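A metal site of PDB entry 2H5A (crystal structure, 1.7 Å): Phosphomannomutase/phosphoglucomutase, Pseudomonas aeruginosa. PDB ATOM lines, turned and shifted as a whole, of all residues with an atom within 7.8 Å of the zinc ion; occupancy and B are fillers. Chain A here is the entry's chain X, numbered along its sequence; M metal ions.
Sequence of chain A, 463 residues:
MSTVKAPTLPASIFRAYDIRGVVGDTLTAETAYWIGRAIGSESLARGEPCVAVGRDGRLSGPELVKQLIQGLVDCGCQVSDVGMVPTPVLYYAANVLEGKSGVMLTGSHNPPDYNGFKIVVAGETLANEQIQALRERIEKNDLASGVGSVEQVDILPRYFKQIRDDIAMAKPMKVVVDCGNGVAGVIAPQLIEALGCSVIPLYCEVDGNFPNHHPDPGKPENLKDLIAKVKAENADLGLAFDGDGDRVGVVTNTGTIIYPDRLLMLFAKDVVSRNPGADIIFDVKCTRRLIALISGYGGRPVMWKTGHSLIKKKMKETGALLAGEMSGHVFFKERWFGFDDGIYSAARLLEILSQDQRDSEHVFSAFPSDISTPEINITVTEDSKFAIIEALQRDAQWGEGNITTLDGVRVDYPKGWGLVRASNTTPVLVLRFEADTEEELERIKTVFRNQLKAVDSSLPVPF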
ATOM      1  N   ARG A  20     -13.342  30.715 -25.542  1.00  0.00           N
ATOM      2  CA  ARG A  20     -12.914  30.509 -24.136  1.00  0.00           C
ATOM      3  C   ARG A  20     -14.081  30.715 -23.185  1.00  0.00           C
ATOM      4  O   ARG A  20     -14.857  31.655 -23.319  1.00  0.00           O
ATOM      5  CB  ARG A  20     -11.733  31.411 -23.747  1.00  0.00           C
ATOM      6  CG  ARG A  20     -11.566  32.683 -24.576  1.00  0.00           C
ATOM      7  CD  ARG A  20     -10.890  33.838 -23.793  1.00  0.00           C
ATOM      8  NE  ARG A  20      -9.528  33.502 -23.379  1.00  0.00           N
ATOM      9  CZ  ARG A  20      -8.459  33.510 -24.172  1.00  0.00           C
ATOM     10  NH1 ARG A  20      -8.573  33.831 -25.456  1.00  0.00           N
ATOM     11  NH2 ARG A  20      -7.257  33.207 -23.674  1.00  0.00           N
ATOM     12  N   THR A  87      -0.366  22.601 -26.788  1.00  0.00           N
ATOM     13  CA  THR A  87      -0.932  23.300 -27.927  1.00  0.00           C
ATOM     14  C   THR A  87      -0.043  23.268 -29.191  1.00  0.00           C
ATOM     15  O   THR A  87      -0.539  22.916 -30.266  1.00  0.00           O
ATOM     16  CB  THR A  87      -1.290  24.754 -27.536  1.00  0.00           C
ATOM     17  OG1 THR A  87      -2.423  24.734 -26.648  1.00  0.00           O
ATOM     18  CG2 THR A  87      -1.644  25.568 -28.782  1.00  0.00           C
ATOM     19  N   PRO A  88       1.259  23.640 -29.075  1.00  0.00           N
ATOM     20  CA  PRO A  88       2.092  23.590 -30.265  1.00  0.00           C
ATOM     21  C   PRO A  88       2.208  22.203 -30.925  1.00  0.00           C
ATOM     22  O   PRO A  88       2.480  22.126 -32.117  1.00  0.00           O
ATOM     23  CB  PRO A  88       3.451  24.070 -29.774  1.00  0.00           C
ATOM     24  CG  PRO A  88       3.461  23.764 -28.308  1.00  0.00           C
ATOM     25  CD  PRO A  88       2.044  24.131 -27.921  1.00  0.00           C
ATOM     26  N   TYR A  91      -0.742  22.059 -33.159  1.00  0.00           N
ATOM     27  CA  TYR A  91      -0.411  22.823 -34.356  1.00  0.00           C
ATOM     28  C   TYR A  91       0.563  22.067 -35.273  1.00  0.00           C
ATOM     29  O   TYR A  91       0.417  22.094 -36.493  1.00  0.00           O
ATOM     30  CB  TYR A  91       0.218  24.176 -34.012  1.00  0.00           C
ATOM     31  CG  TYR A  91      -0.626  25.152 -33.202  1.00  0.00           C
ATOM     32  CD1 TYR A  91      -2.015  25.114 -33.244  1.00  0.00           C
ATOM     33  CD2 TYR A  91      -0.012  26.148 -32.431  1.00  0.00           C
ATOM     34  CE1 TYR A  91      -2.795  26.022 -32.519  1.00  0.00           C
ATOM     35  CE2 TYR A  91      -0.772  27.060 -31.693  1.00  0.00           C
ATOM     36  CZ  TYR A  91      -2.170  26.999 -31.755  1.00  0.00           C
ATOM     37  OH  TYR A  91      -2.958  27.884 -31.050  1.00  0.00           O
ATOM     38  N   THR A 106      -8.249  23.721 -25.009  1.00  0.00           N
ATOM     39  CA  THR A 106      -7.398  24.288 -23.960  1.00  0.00           C
ATOM     40  C   THR A 106      -7.957  25.529 -23.267  1.00  0.00           C
ATOM     41  O   THR A 106      -8.653  26.345 -23.895  1.00  0.00           O
ATOM     42  CB  THR A 106      -5.980  24.607 -24.484  1.00  0.00           C
ATOM     43  OG1 THR A 106      -5.173  25.055 -23.400  1.00  0.00           O
ATOM     44  CG2 THR A 106      -6.003  25.659 -25.593  1.00  0.00           C
ATOM     45  N   GLY A 107      -7.644  25.646 -21.968  1.00  0.00           N
ATOM     46  CA  GLY A 107      -7.943  26.852 -21.186  1.00  0.00           C
ATOM     47  C   GLY A 107      -6.706  27.711 -20.983  1.00  0.00           C
ATOM     48  O   GLY A 107      -6.689  28.595 -20.123  1.00  0.00           O
ATOM     49  N   SEP A 108      -5.655  27.454 -21.770  1.00  0.00           N
ATOM     50  CA  SEP A 108      -4.421  28.263 -21.762  1.00  0.00           C
ATOM     51  CB  SEP A 108      -4.661  29.610 -22.470  1.00  0.00           C
ATOM     52  OG  SEP A 108      -3.542  30.480 -22.374  1.00  0.00           O
ATOM     53  C   SEP A 108      -3.844  28.425 -20.328  1.00  0.00           C
ATOM     54  O   SEP A 108      -3.558  27.424 -19.666  1.00  0.00           O
ATOM     55  P   SEP A 108      -3.218  31.323 -23.716  1.00  0.00           P
ATOM     56  O1P SEP A 108      -2.909  32.838 -23.336  1.00  0.00           O
ATOM     57  O2P SEP A 108      -4.376  31.266 -24.823  1.00  0.00           O
ATOM     58  O3P SEP A 108      -1.913  30.681 -24.391  1.00  0.00           O
ATOM     59  N   HIS A 109      -3.709  29.658 -19.865  1.00  0.00           N
ATOM     60  CA  HIS A 109      -3.062  29.938 -18.567  1.00  0.00           C
ATOM     61  C   HIS A 109      -4.074  30.177 -17.448  1.00  0.00           C
ATOM     62  O   HIS A 109      -3.698  30.467 -16.302  1.00  0.00           O
ATOM     63  CB  HIS A 109      -2.127  31.146 -18.705  1.00  0.00           C
ATOM     64  CG  HIS A 109      -2.839  32.448 -18.901  1.00  0.00           C
ATOM     65  ND1 HIS A 109      -3.202  32.925 -20.138  1.00  0.00           N
ATOM     66  CD2 HIS A 109      -3.269  33.371 -18.001  1.00  0.00           C
ATOM     67  CE1 HIS A 109      -3.820  34.081 -20.006  1.00  0.00           C
ATOM     68  NE2 HIS A 109      -3.872  34.381 -18.713  1.00  0.00           N
ATOM     69  N   ASN A 110      -5.366  30.047 -17.781  1.00  0.00           N
ATOM     70  CA  ASN A 110      -6.451  30.398 -16.862  1.00  0.00           C
ATOM     71  C   ASN A 110      -6.674  29.380 -15.737  1.00  0.00           C
ATOM     72  O   ASN A 110      -6.139  28.274 -15.797  1.00  0.00           O
ATOM     73  CB  ASN A 110      -7.736  30.593 -17.663  1.00  0.00           C
ATOM     74  CG  ASN A 110      -7.668  31.822 -18.556  1.00  0.00           C
ATOM     75  OD1 ASN A 110      -7.768  31.719 -19.780  1.00  0.00           O
ATOM     76  ND2 ASN A 110      -7.487  32.987 -17.957  1.00  0.00           N
ATOM     77  N   LYS A 118      -8.784  26.465 -29.591  1.00  0.00           N
ATOM     78  CA  LYS A 118      -7.963  27.200 -30.539  1.00  0.00           C
ATOM     79  C   LYS A 118      -8.076  26.430 -31.853  1.00  0.00           C
ATOM     80  O   LYS A 118      -7.967  25.195 -31.853  1.00  0.00           O
ATOM     81  CB  LYS A 118      -6.517  27.298 -30.042  1.00  0.00           C
ATOM     82  CG  LYS A 118      -6.389  28.230 -28.856  1.00  0.00           C
ATOM     83  CD  LYS A 118      -5.023  28.131 -28.212  1.00  0.00           C
ATOM     84  CE  LYS A 118      -4.948  29.085 -27.025  1.00  0.00           C
ATOM     85  NZ  LYS A 118      -3.547  29.283 -26.565  1.00  0.00           N
ATOM     86  N   PRO A 215      -0.382  28.394 -13.943  1.00  0.00           N
ATOM     87  CA  PRO A 215       0.626  28.214 -14.994  1.00  0.00           C
ATOM     88  C   PRO A 215       0.625  29.403 -15.953  1.00  0.00           C
ATOM     89  O   PRO A 215       0.175  29.311 -17.098  1.00  0.00           O
ATOM     90  CB  PRO A 215       0.185  26.907 -15.681  1.00  0.00           C
ATOM     91  CG  PRO A 215      -1.297  26.832 -15.455  1.00  0.00           C
ATOM     92  CD  PRO A 215      -1.638  27.658 -14.223  1.00  0.00           C
ATOM     93  N   PRO A 217       3.456  32.238 -16.780  1.00  0.00           N
ATOM     94  CA  PRO A 217       4.811  32.768 -16.624  1.00  0.00           C
ATOM     95  C   PRO A 217       4.948  34.264 -16.902  1.00  0.00           C
ATOM     96  O   PRO A 217       6.040  34.812 -16.741  1.00  0.00           O
ATOM     97  CB  PRO A 217       5.625  31.959 -17.645  1.00  0.00           C
ATOM     98  CG  PRO A 217       4.636  31.604 -18.697  1.00  0.00           C
ATOM     99  CD  PRO A 217       3.350  31.366 -17.970  1.00  0.00           C
ATOM    100  N   PHE A 241       6.787  27.389 -18.409  1.00  0.00           N
ATOM    101  CA  PHE A 241       5.800  27.268 -19.479  1.00  0.00           C
ATOM    102  C   PHE A 241       4.406  27.587 -18.948  1.00  0.00           C
ATOM    103  O   PHE A 241       4.140  27.365 -17.757  1.00  0.00           O
ATOM    104  CB  PHE A 241       5.859  25.869 -20.085  1.00  0.00           C
ATOM    105  CG  PHE A 241       7.198  25.554 -20.699  1.00  0.00           C
ATOM    106  CD1 PHE A 241       7.572  26.116 -21.924  1.00  0.00           C
ATOM    107  CD2 PHE A 241       8.106  24.744 -20.031  1.00  0.00           C
ATOM    108  CE1 PHE A 241       8.825  25.864 -22.479  1.00  0.00           C
ATOM    109  CE2 PHE A 241       9.361  24.478 -20.585  1.00  0.00           C
ATOM    110  CZ  PHE A 241       9.725  25.046 -21.803  1.00  0.00           C
ATOM    111  N   ASP A 242       3.532  28.116 -19.797  1.00  0.00           N
ATOM    112  CA  ASP A 242       2.150  28.289 -19.402  1.00  0.00           C
ATOM    113  C   ASP A 242       1.421  26.948 -19.487  1.00  0.00           C
ATOM    114  O   ASP A 242       2.051  25.928 -19.839  1.00  0.00           O
ATOM    115  CB  ASP A 242       1.428  29.433 -20.150  1.00  0.00           C
ATOM    116  CG  ASP A 242       0.960  29.050 -21.557  1.00  0.00           C
ATOM    117  OD1 ASP A 242       1.530  28.154 -22.209  1.00  0.00           O
ATOM    118  OD2 ASP A 242      -0.001  29.711 -22.025  1.00  0.00           O
ATOM    119  N   GLY A 243       0.137  26.945 -19.146  1.00  0.00           N
ATOM    120  CA  GLY A 243      -0.633  25.700 -19.013  1.00  0.00           C
ATOM    121  C   GLY A 243      -0.621  24.771 -20.220  1.00  0.00           C
ATOM    122  O   GLY A 243      -0.584  23.541 -20.053  1.00  0.00           O
ATOM    123  N   ASP A 244      -0.630  25.343 -21.428  1.00  0.00           N
ATOM    124  CA  ASP A 244      -0.700  24.566 -22.673  1.00  0.00           C
ATOM    125  C   ASP A 244       0.588  24.579 -23.511  1.00  0.00           C
ATOM    126  O   ASP A 244       0.644  23.994 -24.600  1.00  0.00           O
ATOM    127  CB  ASP A 244      -1.933  24.988 -23.507  1.00  0.00           C
ATOM    128  CG  ASP A 244      -1.920  26.449 -23.934  1.00  0.00           C
ATOM    129  OD1 ASP A 244      -1.341  27.289 -23.218  1.00  0.00           O
ATOM    130  OD2 ASP A 244      -2.526  26.768 -24.976  1.00  0.00           O
ATOM    131  N   GLY A 245       1.634  25.234 -22.999  1.00  0.00           N
ATOM    132  CA  GLY A 245       2.961  25.182 -23.602  1.00  0.00           C
ATOM    133  C   GLY A 245       3.226  26.074 -24.808  1.00  0.00           C
ATOM    134  O   GLY A 245       4.258  25.933 -25.472  1.00  0.00           O
ATOM    135  N   ASP A 246       2.339  27.030 -25.073  1.00  0.00           N
ATOM    136  CA  ASP A 246       2.594  27.953 -26.195  1.00  0.00           C
ATOM    137  C   ASP A 246       3.223  29.266 -25.764  1.00  0.00           C
ATOM    138  O   ASP A 246       3.469  30.126 -26.614  1.00  0.00           O
ATOM    139  CB  ASP A 246       1.360  28.201 -27.064  1.00  0.00           C
ATOM    140  CG  ASP A 246       0.190  28.771 -26.286  1.00  0.00           C
ATOM    141  OD1 ASP A 246       0.291  29.031 -25.069  1.00  0.00           O
ATOM    142  OD2 ASP A 246      -0.880  28.944 -26.897  1.00  0.00           O
ATOM    143  N   ARG A 247       3.452  29.416 -24.463  1.00  0.00           N
ATOM    144  CA  ARG A 247       4.155  30.580 -23.909  1.00  0.00           C
ATOM    145  C   ARG A 247       5.326  30.094 -23.068  1.00  0.00           C
ATOM    146  O   ARG A 247       5.268  28.990 -22.471  1.00  0.00           O
ATOM    147  CB  ARG A 247       3.220  31.418 -23.032  1.00  0.00           C
ATOM    148  CG  ARG A 247       2.039  32.020 -23.792  1.00  0.00           C
ATOM    149  CD  ARG A 247       1.406  33.156 -23.006  1.00  0.00           C
ATOM    150  NE  ARG A 247       1.108  32.779 -21.637  1.00  0.00           N
ATOM    151  CZ  ARG A 247       0.688  33.634 -20.706  1.00  0.00           C
ATOM    152  NH1 ARG A 247       0.507  34.919 -20.989  1.00  0.00           N
ATOM    153  NH2 ARG A 247       0.451  33.188 -19.479  1.00  0.00           N
ATOM    154  N   VAL A 248       6.391  30.882 -23.038  1.00  0.00           N
ATOM    155  CA  VAL A 248       7.579  30.560 -22.269  1.00  0.00           C
ATOM    156  C   VAL A 248       7.989  31.817 -21.500  1.00  0.00           C
ATOM    157  O   VAL A 248       7.778  32.933 -22.001  1.00  0.00           O
ATOM    158  CB  VAL A 248       8.735  30.048 -23.170  1.00  0.00           C
ATOM    159  CG1 VAL A 248       9.249  31.166 -24.100  1.00  0.00           C
ATOM    160  CG2 VAL A 248       9.886  29.480 -22.333  1.00  0.00           C
ATOM    161  N   HIS A 308      -2.324  36.021 -30.277  1.00  0.00           N
ATOM    162  CA  HIS A 308      -1.615  34.947 -30.991  1.00  0.00           C
ATOM    163  C   HIS A 308      -2.178  34.681 -32.399  1.00  0.00           C
ATOM    164  O   HIS A 308      -1.400  34.604 -33.359  1.00  0.00           O
ATOM    165  CB  HIS A 308      -1.557  33.669 -30.136  1.00  0.00           C
ATOM    166  CG  HIS A 308      -2.894  33.087 -29.838  1.00  0.00           C
ATOM    167  ND1 HIS A 308      -3.481  32.115 -30.619  1.00  0.00           N
ATOM    168  CD2 HIS A 308      -3.781  33.337 -28.838  1.00  0.00           C
ATOM    169  CE1 HIS A 308      -4.656  31.782 -30.119  1.00  0.00           C
ATOM    170  NE2 HIS A 308      -4.862  32.518 -29.044  1.00  0.00           N
ATOM    171  N   HIS A 329       4.339  34.381 -26.303  1.00  0.00           N
ATOM    172  CA  HIS A 329       4.091  33.599 -27.497  1.00  0.00           C
ATOM    173  C   HIS A 329       5.188  33.959 -28.490  1.00  0.00           C
ATOM    174  O   HIS A 329       5.290  35.112 -28.886  1.00  0.00           O
ATOM    175  CB  HIS A 329       2.737  33.950 -28.103  1.00  0.00           C
ATOM    176  CG  HIS A 329       1.564  33.480 -27.293  1.00  0.00           C
ATOM    177  ND1 HIS A 329       0.932  32.280 -27.523  1.00  0.00           N
ATOM    178  CD2 HIS A 329       0.886  34.084 -26.290  1.00  0.00           C
ATOM    179  CE1 HIS A 329      -0.079  32.152 -26.685  1.00  0.00           C
ATOM    180  NE2 HIS A 329      -0.130  33.224 -25.916  1.00  0.00           N
ATOM    181  N   ASP A 340       3.142  29.520 -32.765  1.00  0.00           N
ATOM    182  CA  ASP A 340       3.701  29.783 -31.441  1.00  0.00           C
ATOM    183  C   ASP A 340       3.967  28.483 -30.694  1.00  0.00           C
ATOM    184  O   ASP A 340       3.160  27.562 -30.723  1.00  0.00           O
ATOM    185  CB  ASP A 340       2.841  30.736 -30.594  1.00  0.00           C
ATOM    186  CG  ASP A 340       1.335  30.467 -30.706  1.00  0.00           C
ATOM    187  OD1 ASP A 340       0.858  30.116 -31.810  1.00  0.00           O
ATOM    188  OD2 ASP A 340       0.630  30.711 -29.700  1.00  0.00           O
HETATM  189 ZN    ZN M   1      -0.951  29.202 -23.688  1.00  0.00          ZN
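The backbone carbonyl oxygen of Asp 246 is in hydrogen-bond range of a ring nitrogen (ND1) of His 329, 3.4 Å away. The backbone NH (N) of Gly 245 is in hydrogen-bond range of the side-chain carboxylate (OD1) of Asp 242, at 3.0 Å. The side-chain amino group of Lys 118 is in salt-bridge range of the side-chain carboxylate of Asp 246 (2.7 Å). O3P of SEP 108 sits close to a ring nitrogen (NE2) of His 329 (3.5 Å). The side-chain carboxylate (OD2) of Asp 244 is in salt-bridge range of the side-chain amino group (NZ) of Lys 118. OD2 of Asp 244 sits at hydrogen-bond distance from OG1 of Thr 87 (2.6 Å). OD1 of Asp 242 sits at hydrogen-bond distance from N of Arg 247, at 3.2 Å. O2P of SEP 108 is in salt-bridge range of NH2 of Arg 20 (3.7 Å).
Merely in contact with the zinc ion: Lys 118. Within 4 Å of the zinc ion: SEP 108, Lys 118, Asp 242, Asp 244 and Asp 246.
The zinc ion is bound by OD1 of Asp 246 (1.9 Å), O3P of SEP 108 (1.9 Å), OD2 of Asp 242 (2.0 Å) and OD1 of Asp 244 (2.0 Å).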
